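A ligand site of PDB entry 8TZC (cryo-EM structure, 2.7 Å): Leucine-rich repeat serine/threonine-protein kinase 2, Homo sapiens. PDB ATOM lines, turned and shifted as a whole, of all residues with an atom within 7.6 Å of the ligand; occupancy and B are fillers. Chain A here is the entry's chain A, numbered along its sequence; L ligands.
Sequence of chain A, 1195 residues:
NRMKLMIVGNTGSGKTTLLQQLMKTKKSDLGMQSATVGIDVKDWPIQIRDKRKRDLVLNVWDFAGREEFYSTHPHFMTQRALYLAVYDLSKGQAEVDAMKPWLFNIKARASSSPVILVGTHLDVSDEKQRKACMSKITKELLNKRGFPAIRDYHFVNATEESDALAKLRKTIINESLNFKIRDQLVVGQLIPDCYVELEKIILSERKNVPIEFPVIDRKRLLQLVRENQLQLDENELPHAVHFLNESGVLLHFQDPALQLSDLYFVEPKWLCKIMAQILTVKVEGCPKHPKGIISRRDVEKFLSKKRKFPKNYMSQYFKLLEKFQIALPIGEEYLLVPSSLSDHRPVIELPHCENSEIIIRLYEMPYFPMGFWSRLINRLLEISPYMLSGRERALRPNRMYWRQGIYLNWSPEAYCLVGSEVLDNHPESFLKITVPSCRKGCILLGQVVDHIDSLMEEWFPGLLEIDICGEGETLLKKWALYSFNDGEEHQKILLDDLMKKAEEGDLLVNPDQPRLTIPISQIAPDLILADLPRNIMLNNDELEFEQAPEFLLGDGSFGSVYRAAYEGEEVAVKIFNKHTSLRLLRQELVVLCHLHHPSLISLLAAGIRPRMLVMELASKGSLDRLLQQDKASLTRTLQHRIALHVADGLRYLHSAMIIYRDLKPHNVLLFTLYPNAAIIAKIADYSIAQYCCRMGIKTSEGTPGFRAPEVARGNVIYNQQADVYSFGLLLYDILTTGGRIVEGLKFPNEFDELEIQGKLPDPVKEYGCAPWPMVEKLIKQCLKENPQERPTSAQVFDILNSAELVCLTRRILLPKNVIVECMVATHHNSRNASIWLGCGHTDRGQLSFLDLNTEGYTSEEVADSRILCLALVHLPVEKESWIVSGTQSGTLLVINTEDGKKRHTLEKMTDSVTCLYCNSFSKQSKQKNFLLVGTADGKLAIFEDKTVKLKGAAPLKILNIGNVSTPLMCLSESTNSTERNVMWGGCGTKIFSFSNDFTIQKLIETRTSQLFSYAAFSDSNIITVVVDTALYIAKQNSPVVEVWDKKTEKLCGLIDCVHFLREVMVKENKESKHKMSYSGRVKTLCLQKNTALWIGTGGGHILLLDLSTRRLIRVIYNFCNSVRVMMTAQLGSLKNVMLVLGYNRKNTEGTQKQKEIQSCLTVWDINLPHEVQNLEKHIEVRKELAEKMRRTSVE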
ATOM      1  N   ILE A   7      25.603 -26.700  34.335  1.00  0.00           N
ATOM      2  CA  ILE A   7      25.324 -27.544  33.180  1.00  0.00           C
ATOM      3  C   ILE A   7      25.566 -26.672  31.956  1.00  0.00           C
ATOM      4  O   ILE A   7      24.736 -25.806  31.631  1.00  0.00           O
ATOM      5  CB  ILE A   7      23.899 -28.111  33.203  1.00  0.00           C
ATOM      6  CG1 ILE A   7      23.705 -28.986  34.438  1.00  0.00           C
ATOM      7  CG2 ILE A   7      23.636 -28.920  31.949  1.00  0.00           C
ATOM      8  CD1 ILE A   7      22.398 -29.744  34.449  1.00  0.00           C
ATOM      9  N   GLY A   9      27.041 -26.120  27.775  1.00  0.00           N
ATOM     10  CA  GLY A   9      27.035 -26.752  26.467  1.00  0.00           C
ATOM     11  C   GLY A   9      26.480 -25.813  25.421  1.00  0.00           C
ATOM     12  O   GLY A   9      26.026 -24.700  25.713  1.00  0.00           O
ATOM     13  N   ASN A  10      26.507 -26.291  24.178  1.00  0.00           N
ATOM     14  CA  ASN A  10      25.999 -25.520  23.067  1.00  0.00           C
ATOM     15  C   ASN A  10      24.467 -25.509  23.066  1.00  0.00           C
ATOM     16  O   ASN A  10      23.813 -26.304  23.752  1.00  0.00           O
ATOM     17  CB  ASN A  10      26.511 -26.078  21.741  1.00  0.00           C
ATOM     18  CG  ASN A  10      27.781 -25.397  21.269  1.00  0.00           C
ATOM     19  OD1 ASN A  10      28.221 -24.415  21.863  1.00  0.00           O
ATOM     20  ND2 ASN A  10      28.360 -25.901  20.191  1.00  0.00           N
ATOM     21  N   THR A  11      23.902 -24.581  22.302  1.00  0.00           N
ATOM     22  CA  THR A  11      22.453 -24.454  22.229  1.00  0.00           C
ATOM     23  C   THR A  11      21.836 -25.704  21.613  1.00  0.00           C
ATOM     24  O   THR A  11      22.368 -26.288  20.656  1.00  0.00           O
ATOM     25  CB  THR A  11      22.066 -23.222  21.414  1.00  0.00           C
ATOM     26  OG1 THR A  11      20.656 -23.248  21.141  1.00  0.00           O
ATOM     27  CG2 THR A  11      22.838 -23.173  20.104  1.00  0.00           C
ATOM     28  N   GLY A  12      20.698 -26.125  22.168  1.00  0.00           N
ATOM     29  CA  GLY A  12      20.022 -27.320  21.696  1.00  0.00           C
ATOM     30  C   GLY A  12      20.659 -28.620  22.101  1.00  0.00           C
ATOM     31  O   GLY A  12      20.223 -29.673  21.622  1.00  0.00           O
ATOM     32  N   SER A  13      21.679 -28.592  22.964  1.00  0.00           N
ATOM     33  CA  SER A  13      22.332 -29.824  23.381  1.00  0.00           C
ATOM     34  C   SER A  13      21.384 -30.716  24.171  1.00  0.00           C
ATOM     35  O   SER A  13      21.365 -31.940  23.972  1.00  0.00           O
ATOM     36  CB  SER A  13      23.582 -29.499  24.199  1.00  0.00           C
ATOM     37  OG  SER A  13      24.463 -30.611  24.242  1.00  0.00           O
ATOM     38  N   GLY A  14      20.594 -30.129  25.065  1.00  0.00           N
ATOM     39  CA  GLY A  14      19.672 -30.910  25.870  1.00  0.00           C
ATOM     40  C   GLY A  14      19.642 -30.492  27.321  1.00  0.00           C
ATOM     41  O   GLY A  14      18.948 -31.111  28.140  1.00  0.00           O
ATOM     42  N   LYS A  15      20.375 -29.442  27.670  1.00  0.00           N
ATOM     43  CA  LYS A  15      20.426 -28.942  29.037  1.00  0.00           C
ATOM     44  C   LYS A  15      19.078 -28.365  29.457  1.00  0.00           C
ATOM     45  O   LYS A  15      18.546 -28.721  30.507  1.00  0.00           O
ATOM     46  CB  LYS A  15      21.515 -27.873  29.183  1.00  0.00           C
ATOM     47  CG  LYS A  15      22.753 -28.140  28.338  1.00  0.00           C
ATOM     48  CD  LYS A  15      23.662 -26.923  28.308  1.00  0.00           C
ATOM     49  CE  LYS A  15      22.970 -25.736  27.684  1.00  0.00           C
ATOM     50  NZ  LYS A  15      22.522 -26.009  26.295  1.00  0.00           N
ATOM     51  N   THR A  17      16.329 -30.171  29.231  1.00  0.00           N
ATOM     52  CA  THR A  17      15.695 -31.460  28.965  1.00  0.00           C
ATOM     53  C   THR A  17      16.456 -32.591  29.662  1.00  0.00           C
ATOM     54  O   THR A  17      15.947 -33.698  29.812  1.00  0.00           O
ATOM     55  CB  THR A  17      15.621 -31.746  27.457  1.00  0.00           C
ATOM     56  OG1 THR A  17      15.387 -30.518  26.760  1.00  0.00           O
ATOM     57  CG2 THR A  17      14.478 -32.703  27.158  1.00  0.00           C
ATOM     58  N   LEU A  18      17.687 -32.298  30.077  1.00  0.00           N
ATOM     59  CA  LEU A  18      18.487 -33.227  30.877  1.00  0.00           C
ATOM     60  C   LEU A  18      18.416 -32.915  32.361  1.00  0.00           C
ATOM     61  O   LEU A  18      18.316 -33.832  33.175  1.00  0.00           O
ATOM     62  CB  LEU A  18      19.941 -33.210  30.413  1.00  0.00           C
ATOM     63  CG  LEU A  18      20.981 -33.810  31.365  1.00  0.00           C
ATOM     64  CD1 LEU A  18      21.032 -35.320  31.203  1.00  0.00           C
ATOM     65  CD2 LEU A  18      22.349 -33.200  31.119  1.00  0.00           C
ATOM     66  N   LEU A  19      18.442 -31.631  32.724  1.00  0.00           N
ATOM     67  CA  LEU A  19      18.330 -31.250  34.124  1.00  0.00           C
ATOM     68  C   LEU A  19      16.982 -31.673  34.702  1.00  0.00           C
ATOM     69  O   LEU A  19      16.900 -32.153  35.836  1.00  0.00           O
ATOM     70  CB  LEU A  19      18.530 -29.744  34.274  1.00  0.00           C
ATOM     71  CG  LEU A  19      18.107 -29.121  35.605  1.00  0.00           C
ATOM     72  CD1 LEU A  19      19.027 -29.587  36.724  1.00  0.00           C
ATOM     73  CD2 LEU A  19      18.115 -27.600  35.496  1.00  0.00           C
ATOM     74  N   GLN A  20      15.905 -31.497  33.921  1.00  0.00           N
ATOM     75  CA  GLN A  20      14.573 -31.868  34.395  1.00  0.00           C
ATOM     76  C   GLN A  20      14.491 -33.351  34.711  1.00  0.00           C
ATOM     77  O   GLN A  20      13.916 -33.750  35.743  1.00  0.00           O
ATOM     78  CB  GLN A  20      13.518 -31.470  33.368  1.00  0.00           C
ATOM     79  CG  GLN A  20      13.452 -29.976  33.100  1.00  0.00           C
ATOM     80  CD  GLN A  20      12.553 -29.637  31.927  1.00  0.00           C
ATOM     81  OE1 GLN A  20      11.983 -30.522  31.290  1.00  0.00           O
ATOM     82  NE2 GLN A  20      12.426 -28.349  31.636  1.00  0.00           N
ATOM     83  N   ALA A  35      14.745 -22.838  24.605  1.00  0.00           N
ATOM     84  CA  ALA A  35      16.015 -22.139  24.710  1.00  0.00           C
ATOM     85  C   ALA A  35      16.010 -21.178  25.897  1.00  0.00           C
ATOM     86  O   ALA A  35      15.314 -20.157  25.877  1.00  0.00           O
ATOM     87  CB  ALA A  35      16.305 -21.382  23.420  1.00  0.00           C
ATOM     88  N   THR A  36      16.770 -21.515  26.925  1.00  0.00           N
ATOM     89  CA  THR A  36      16.834 -20.685  28.122  1.00  0.00           C
ATOM     90  C   THR A  36      17.512 -19.351  27.815  1.00  0.00           C
ATOM     91  O   THR A  36      18.412 -19.258  26.965  1.00  0.00           O
ATOM     92  CB  THR A  36      17.588 -21.399  29.245  1.00  0.00           C
ATOM     93  OG1 THR A  36      18.992 -21.138  29.118  1.00  0.00           O
ATOM     94  CG2 THR A  36      17.337 -22.900  29.175  1.00  0.00           C
ATOM     95  N   VAL A  37      17.072 -18.314  28.513  1.00  0.00           N
ATOM     96  CA  VAL A  37      17.608 -16.964  28.375  1.00  0.00           C
ATOM     97  C   VAL A  37      18.448 -16.674  29.608  1.00  0.00           C
ATOM     98  O   VAL A  37      17.984 -16.837  30.741  1.00  0.00           O
ATOM     99  CB  VAL A  37      16.492 -15.924  28.213  1.00  0.00           C
ATOM    100  CG1 VAL A  37      17.056 -14.513  28.290  1.00  0.00           C
ATOM    101  CG2 VAL A  37      15.767 -16.131  26.888  1.00  0.00           C
ATOM    102  N   ASP A  40      19.540 -20.216  34.078  1.00  0.00           N
ATOM    103  CA  ASP A  40      18.480 -20.755  34.921  1.00  0.00           C
ATOM    104  C   ASP A  40      19.095 -21.304  36.204  1.00  0.00           C
ATOM    105  O   ASP A  40      19.981 -22.155  36.150  1.00  0.00           O
ATOM    106  CB  ASP A  40      17.710 -21.846  34.192  1.00  0.00           C
ATOM    107  CG  ASP A  40      16.697 -21.289  33.206  1.00  0.00           C
ATOM    108  OD1 ASP A  40      16.298 -20.108  33.359  1.00  0.00           O
ATOM    109  OD2 ASP A  40      16.289 -22.027  32.284  1.00  0.00           O
ATOM    110  N   ASP A  62      21.808 -23.756  35.106  1.00  0.00           N
ATOM    111  CA  ASP A  62      21.679 -24.128  33.696  1.00  0.00           C
ATOM    112  C   ASP A  62      22.050 -22.943  32.818  1.00  0.00           C
ATOM    113  O   ASP A  62      21.369 -21.910  32.844  1.00  0.00           O
ATOM    114  CB  ASP A  62      20.249 -24.599  33.408  1.00  0.00           C
ATOM    115  CG  ASP A  62      20.160 -25.463  32.171  1.00  0.00           C
ATOM    116  OD1 ASP A  62      20.752 -25.090  31.136  1.00  0.00           O
ATOM    117  OD2 ASP A  62      19.498 -26.527  32.229  1.00  0.00           O
ATOM    118  N   PHE A  63      23.119 -23.089  32.057  1.00  0.00           N
ATOM    119  CA  PHE A  63      23.597 -22.022  31.186  1.00  0.00           C
ATOM    120  C   PHE A  63      22.882 -22.072  29.844  1.00  0.00           C
ATOM    121  O   PHE A  63      22.305 -23.087  29.443  1.00  0.00           O
ATOM    122  CB  PHE A  63      25.107 -22.142  30.975  1.00  0.00           C
ATOM    123  CG  PHE A  63      25.923 -21.620  32.129  1.00  0.00           C
ATOM    124  CD1 PHE A  63      26.008 -22.353  33.303  1.00  0.00           C
ATOM    125  CD2 PHE A  63      26.599 -20.423  32.032  1.00  0.00           C
ATOM    126  CE1 PHE A  63      26.751 -21.879  34.366  1.00  0.00           C
ATOM    127  CE2 PHE A  63      27.342 -19.950  33.095  1.00  0.00           C
ATOM    128  CZ  PHE A  63      27.425 -20.679  34.260  1.00  0.00           C
ATOM    129  N   ALA A  64      22.911 -20.947  29.138  1.00  0.00           N
ATOM    130  CA  ALA A  64      22.313 -20.845  27.818  1.00  0.00           C
ATOM    131  C   ALA A  64      23.378 -21.051  26.750  1.00  0.00           C
ATOM    132  O   ALA A  64      24.450 -20.429  26.792  1.00  0.00           O
ATOM    133  CB  ALA A  64      21.641 -19.476  27.633  1.00  0.00           C
ATOM    134  N   GLY A  65      23.093 -21.931  25.801  1.00  0.00           N
ATOM    135  CA  GLY A  65      24.026 -22.248  24.740  1.00  0.00           C
ATOM    136  C   GLY A  65      24.024 -21.286  23.571  1.00  0.00           C
ATOM    137  O   GLY A  65      24.820 -21.461  22.639  1.00  0.00           O
ATOM    138  N   ARG A  66      23.161 -20.282  23.581  1.00  0.00           N
ATOM    139  CA  ARG A  66      23.122 -19.301  22.505  1.00  0.00           C
ATOM    140  C   ARG A  66      24.263 -18.316  22.651  1.00  0.00           C
ATOM    141  O   ARG A  66      24.597 -17.886  23.753  1.00  0.00           O
ATOM    142  CB  ARG A  66      21.769 -18.587  22.487  1.00  0.00           C
ATOM    143  CG  ARG A  66      20.590 -19.537  22.548  1.00  0.00           C
ATOM    144  CD  ARG A  66      19.385 -19.018  21.776  1.00  0.00           C
ATOM    145  NE  ARG A  66      18.361 -18.451  22.647  1.00  0.00           N
ATOM    146  CZ  ARG A  66      18.296 -17.171  22.985  1.00  0.00           C
ATOM    147  NH1 ARG A  66      19.172 -16.290  22.547  1.00  0.00           N
ATOM    148  NH2 ARG A  66      17.310 -16.778  23.791  1.00  0.00           N
ATOM    149  N   PHE A  69      24.847 -14.778  24.966  1.00  0.00           N
ATOM    150  CA  PHE A  69      25.137 -14.727  26.390  1.00  0.00           C
ATOM    151  C   PHE A  69      26.547 -15.200  26.731  1.00  0.00           C
ATOM    152  O   PHE A  69      26.936 -15.148  27.904  1.00  0.00           O
ATOM    153  CB  PHE A  69      24.116 -15.575  27.158  1.00  0.00           C
ATOM    154  CG  PHE A  69      22.730 -15.515  26.575  1.00  0.00           C
ATOM    155  CD1 PHE A  69      21.905 -14.428  26.817  1.00  0.00           C
ATOM    156  CD2 PHE A  69      22.253 -16.546  25.784  1.00  0.00           C
ATOM    157  CE1 PHE A  69      20.637 -14.371  26.283  1.00  0.00           C
ATOM    158  CE2 PHE A  69      20.977 -16.494  25.250  1.00  0.00           C
ATOM    159  CZ  PHE A  69      20.176 -15.408  25.498  1.00  0.00           C
ATOM    160  N   VAL A  86      27.715 -30.738  28.346  1.00  0.00           N
ATOM    161  CA  VAL A  86      26.687 -31.464  27.597  1.00  0.00           C
ATOM    162  C   VAL A  86      26.895 -31.198  26.111  1.00  0.00           C
ATOM    163  O   VAL A  86      26.772 -30.063  25.650  1.00  0.00           O
ATOM    164  CB  VAL A  86      25.278 -31.039  28.037  1.00  0.00           C
ATOM    165  CG1 VAL A  86      24.226 -31.803  27.257  1.00  0.00           C
ATOM    166  CG2 VAL A  86      25.103 -31.264  29.532  1.00  0.00           C
ATOM    167  N   ASP A  88      26.055 -32.841  22.028  1.00  0.00           N
ATOM    168  CA  ASP A  88      25.166 -33.699  21.252  1.00  0.00           C
ATOM    169  C   ASP A  88      25.868 -34.981  20.818  1.00  0.00           C
ATOM    170  O   ASP A  88      27.024 -34.956  20.401  1.00  0.00           O
ATOM    171  CB  ASP A  88      24.637 -32.947  20.029  1.00  0.00           C
ATOM    172  CG  ASP A  88      23.302 -33.490  19.550  1.00  0.00           C
ATOM    173  OD1 ASP A  88      23.198 -34.709  19.338  1.00  0.00           O
ATOM    174  OD2 ASP A  88      22.361 -32.678  19.392  1.00  0.00           O
ATOM    175  N   THR A 120      24.469 -36.338  24.778  1.00  0.00           N
ATOM    176  CA  THR A 120      23.024 -36.424  24.599  1.00  0.00           C
ATOM    177  C   THR A 120      22.667 -36.904  23.198  1.00  0.00           C
ATOM    178  O   THR A 120      22.128 -37.988  23.024  1.00  0.00           O
ATOM    179  CB  THR A 120      22.358 -35.061  24.849  1.00  0.00           C
ATOM    180  OG1 THR A 120      22.774 -34.541  26.122  1.00  0.00           O
ATOM    181  CG2 THR A 120      20.838 -35.204  24.839  1.00  0.00           C
ATOM    182  N   VAL A 156      23.599 -40.234  27.468  1.00  0.00           N
ATOM    183  CA  VAL A 156      22.207 -40.372  27.893  1.00  0.00           C
ATOM    184  C   VAL A 156      21.284 -40.469  26.687  1.00  0.00           C
ATOM    185  O   VAL A 156      21.128 -39.501  25.937  1.00  0.00           O
ATOM    186  CB  VAL A 156      21.789 -39.205  28.811  1.00  0.00           C
ATOM    187  CG1 VAL A 156      20.293 -39.263  29.082  1.00  0.00           C
ATOM    188  CG2 VAL A 156      22.570 -39.243  30.105  1.00  0.00           C
HETATM  189  P1  LIG L   1      19.247 -24.613  25.790  1.00  0.00           P
HETATM  190  O1  LIG L   1      19.269 -24.721  27.298  1.00  0.00           O
HETATM  191  O2  LIG L   1      19.065 -23.175  25.394  1.00  0.00           O
HETATM  192  O3  LIG L   1      20.544 -25.138  25.237  1.00  0.00           O
HETATM  193  O4  LIG L   1      18.028 -25.494  25.208  1.00  0.00           O
HETATM  194  P2  LIG L   1      17.915 -27.044  25.614  1.00  0.00           P
HETATM  195  O5  LIG L   1      17.297 -27.195  26.983  1.00  0.00           O
HETATM  196  O6  LIG L   1      19.272 -27.706  25.564  1.00  0.00           O
HETATM  197  O7  LIG L   1      16.944 -27.681  24.493  1.00  0.00           O
HETATM  198  C1  LIG L   1      16.932 -29.089  24.308  1.00  0.00           C
HETATM  199  C2  LIG L   1      16.033 -29.494  23.152  1.00  0.00           C
HETATM  200  O8  LIG L   1      16.612 -30.627  22.508  1.00  0.00           O
HETATM  201  C3  LIG L   1      14.654 -29.904  23.643  1.00  0.00           C
HETATM  202  O9  LIG L   1      13.658 -29.064  23.071  1.00  0.00           O
HETATM  203  C4  LIG L   1      14.454 -31.341  23.192  1.00  0.00           C
HETATM  204  O10 LIG L   1      13.266 -31.443  22.415  1.00  0.00           O
HETATM  205  C5  LIG L   1      15.671 -31.689  22.353  1.00  0.00           C
HETATM  206  N1  LIG L   1      16.282 -32.949  22.824  1.00  0.00           N
HETATM  207  C6  LIG L   1      17.187 -33.063  23.820  1.00  0.00           C
HETATM  208  N2  LIG L   1      17.552 -34.352  24.004  1.00  0.00           N
HETATM  209  C7  LIG L   1      16.880 -35.099  23.104  1.00  0.00           C
HETATM  210  C8  LIG L   1      16.799 -36.542  22.756  1.00  0.00           C
HETATM  211  O11 LIG L   1      17.479 -37.385  23.374  1.00  0.00           O
HETATM  212  N3  LIG L   1      15.985 -36.903  21.763  1.00  0.00           N
HETATM  213  C9  LIG L   1      15.237 -36.005  21.082  1.00  0.00           C
HETATM  214  N4  LIG L   1      14.429 -36.451  20.088  1.00  0.00           N
HETATM  215  N5  LIG L   1      15.258 -34.671  21.346  1.00  0.00           N
HETATM  216  C10 LIG L   1      16.044 -34.170  22.334  1.00  0.00           C
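O2 of the ligand lies within hydrogen-bond range of N of Thr 36, at 3.2 Å.
The backbone NH (N) of Lys 15 is in hydrogen-bond range of an oxygen (O6) of the ligand (2.9 Å).
The backbone NH (N) of Gly 14 sits at hydrogen-bond distance from an oxygen (O6) of the ligand, at 2.8 Å.
An oxygen (O3) of the ligand is in hydrogen-bond range of the backbone NH (N) of Gly 12 (3.2 Å).
O3 of the ligand is in salt-bridge range of NZ of Lys 15.
N of Thr 11 sits at hydrogen-bond distance from O of Gly 65, 3.3 Å away.
The side-chain amino group (NZ) of Lys 15 sits at hydrogen-bond distance from the backbone carbonyl oxygen (O) of Asn 10, 2.9 Å away.
O of Val 86 is in hydrogen-bond range of OG of Ser 13.
Merely in contact with the ligand: Asn 10, Thr 11, Ser 13, Thr 17, Ala 35 and Thr 120.
Hydrophobic or aromatic side chains that line the ligand: Ala 35.
Of the 26 residues printed, 10 come within 4 Å of the ligand.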
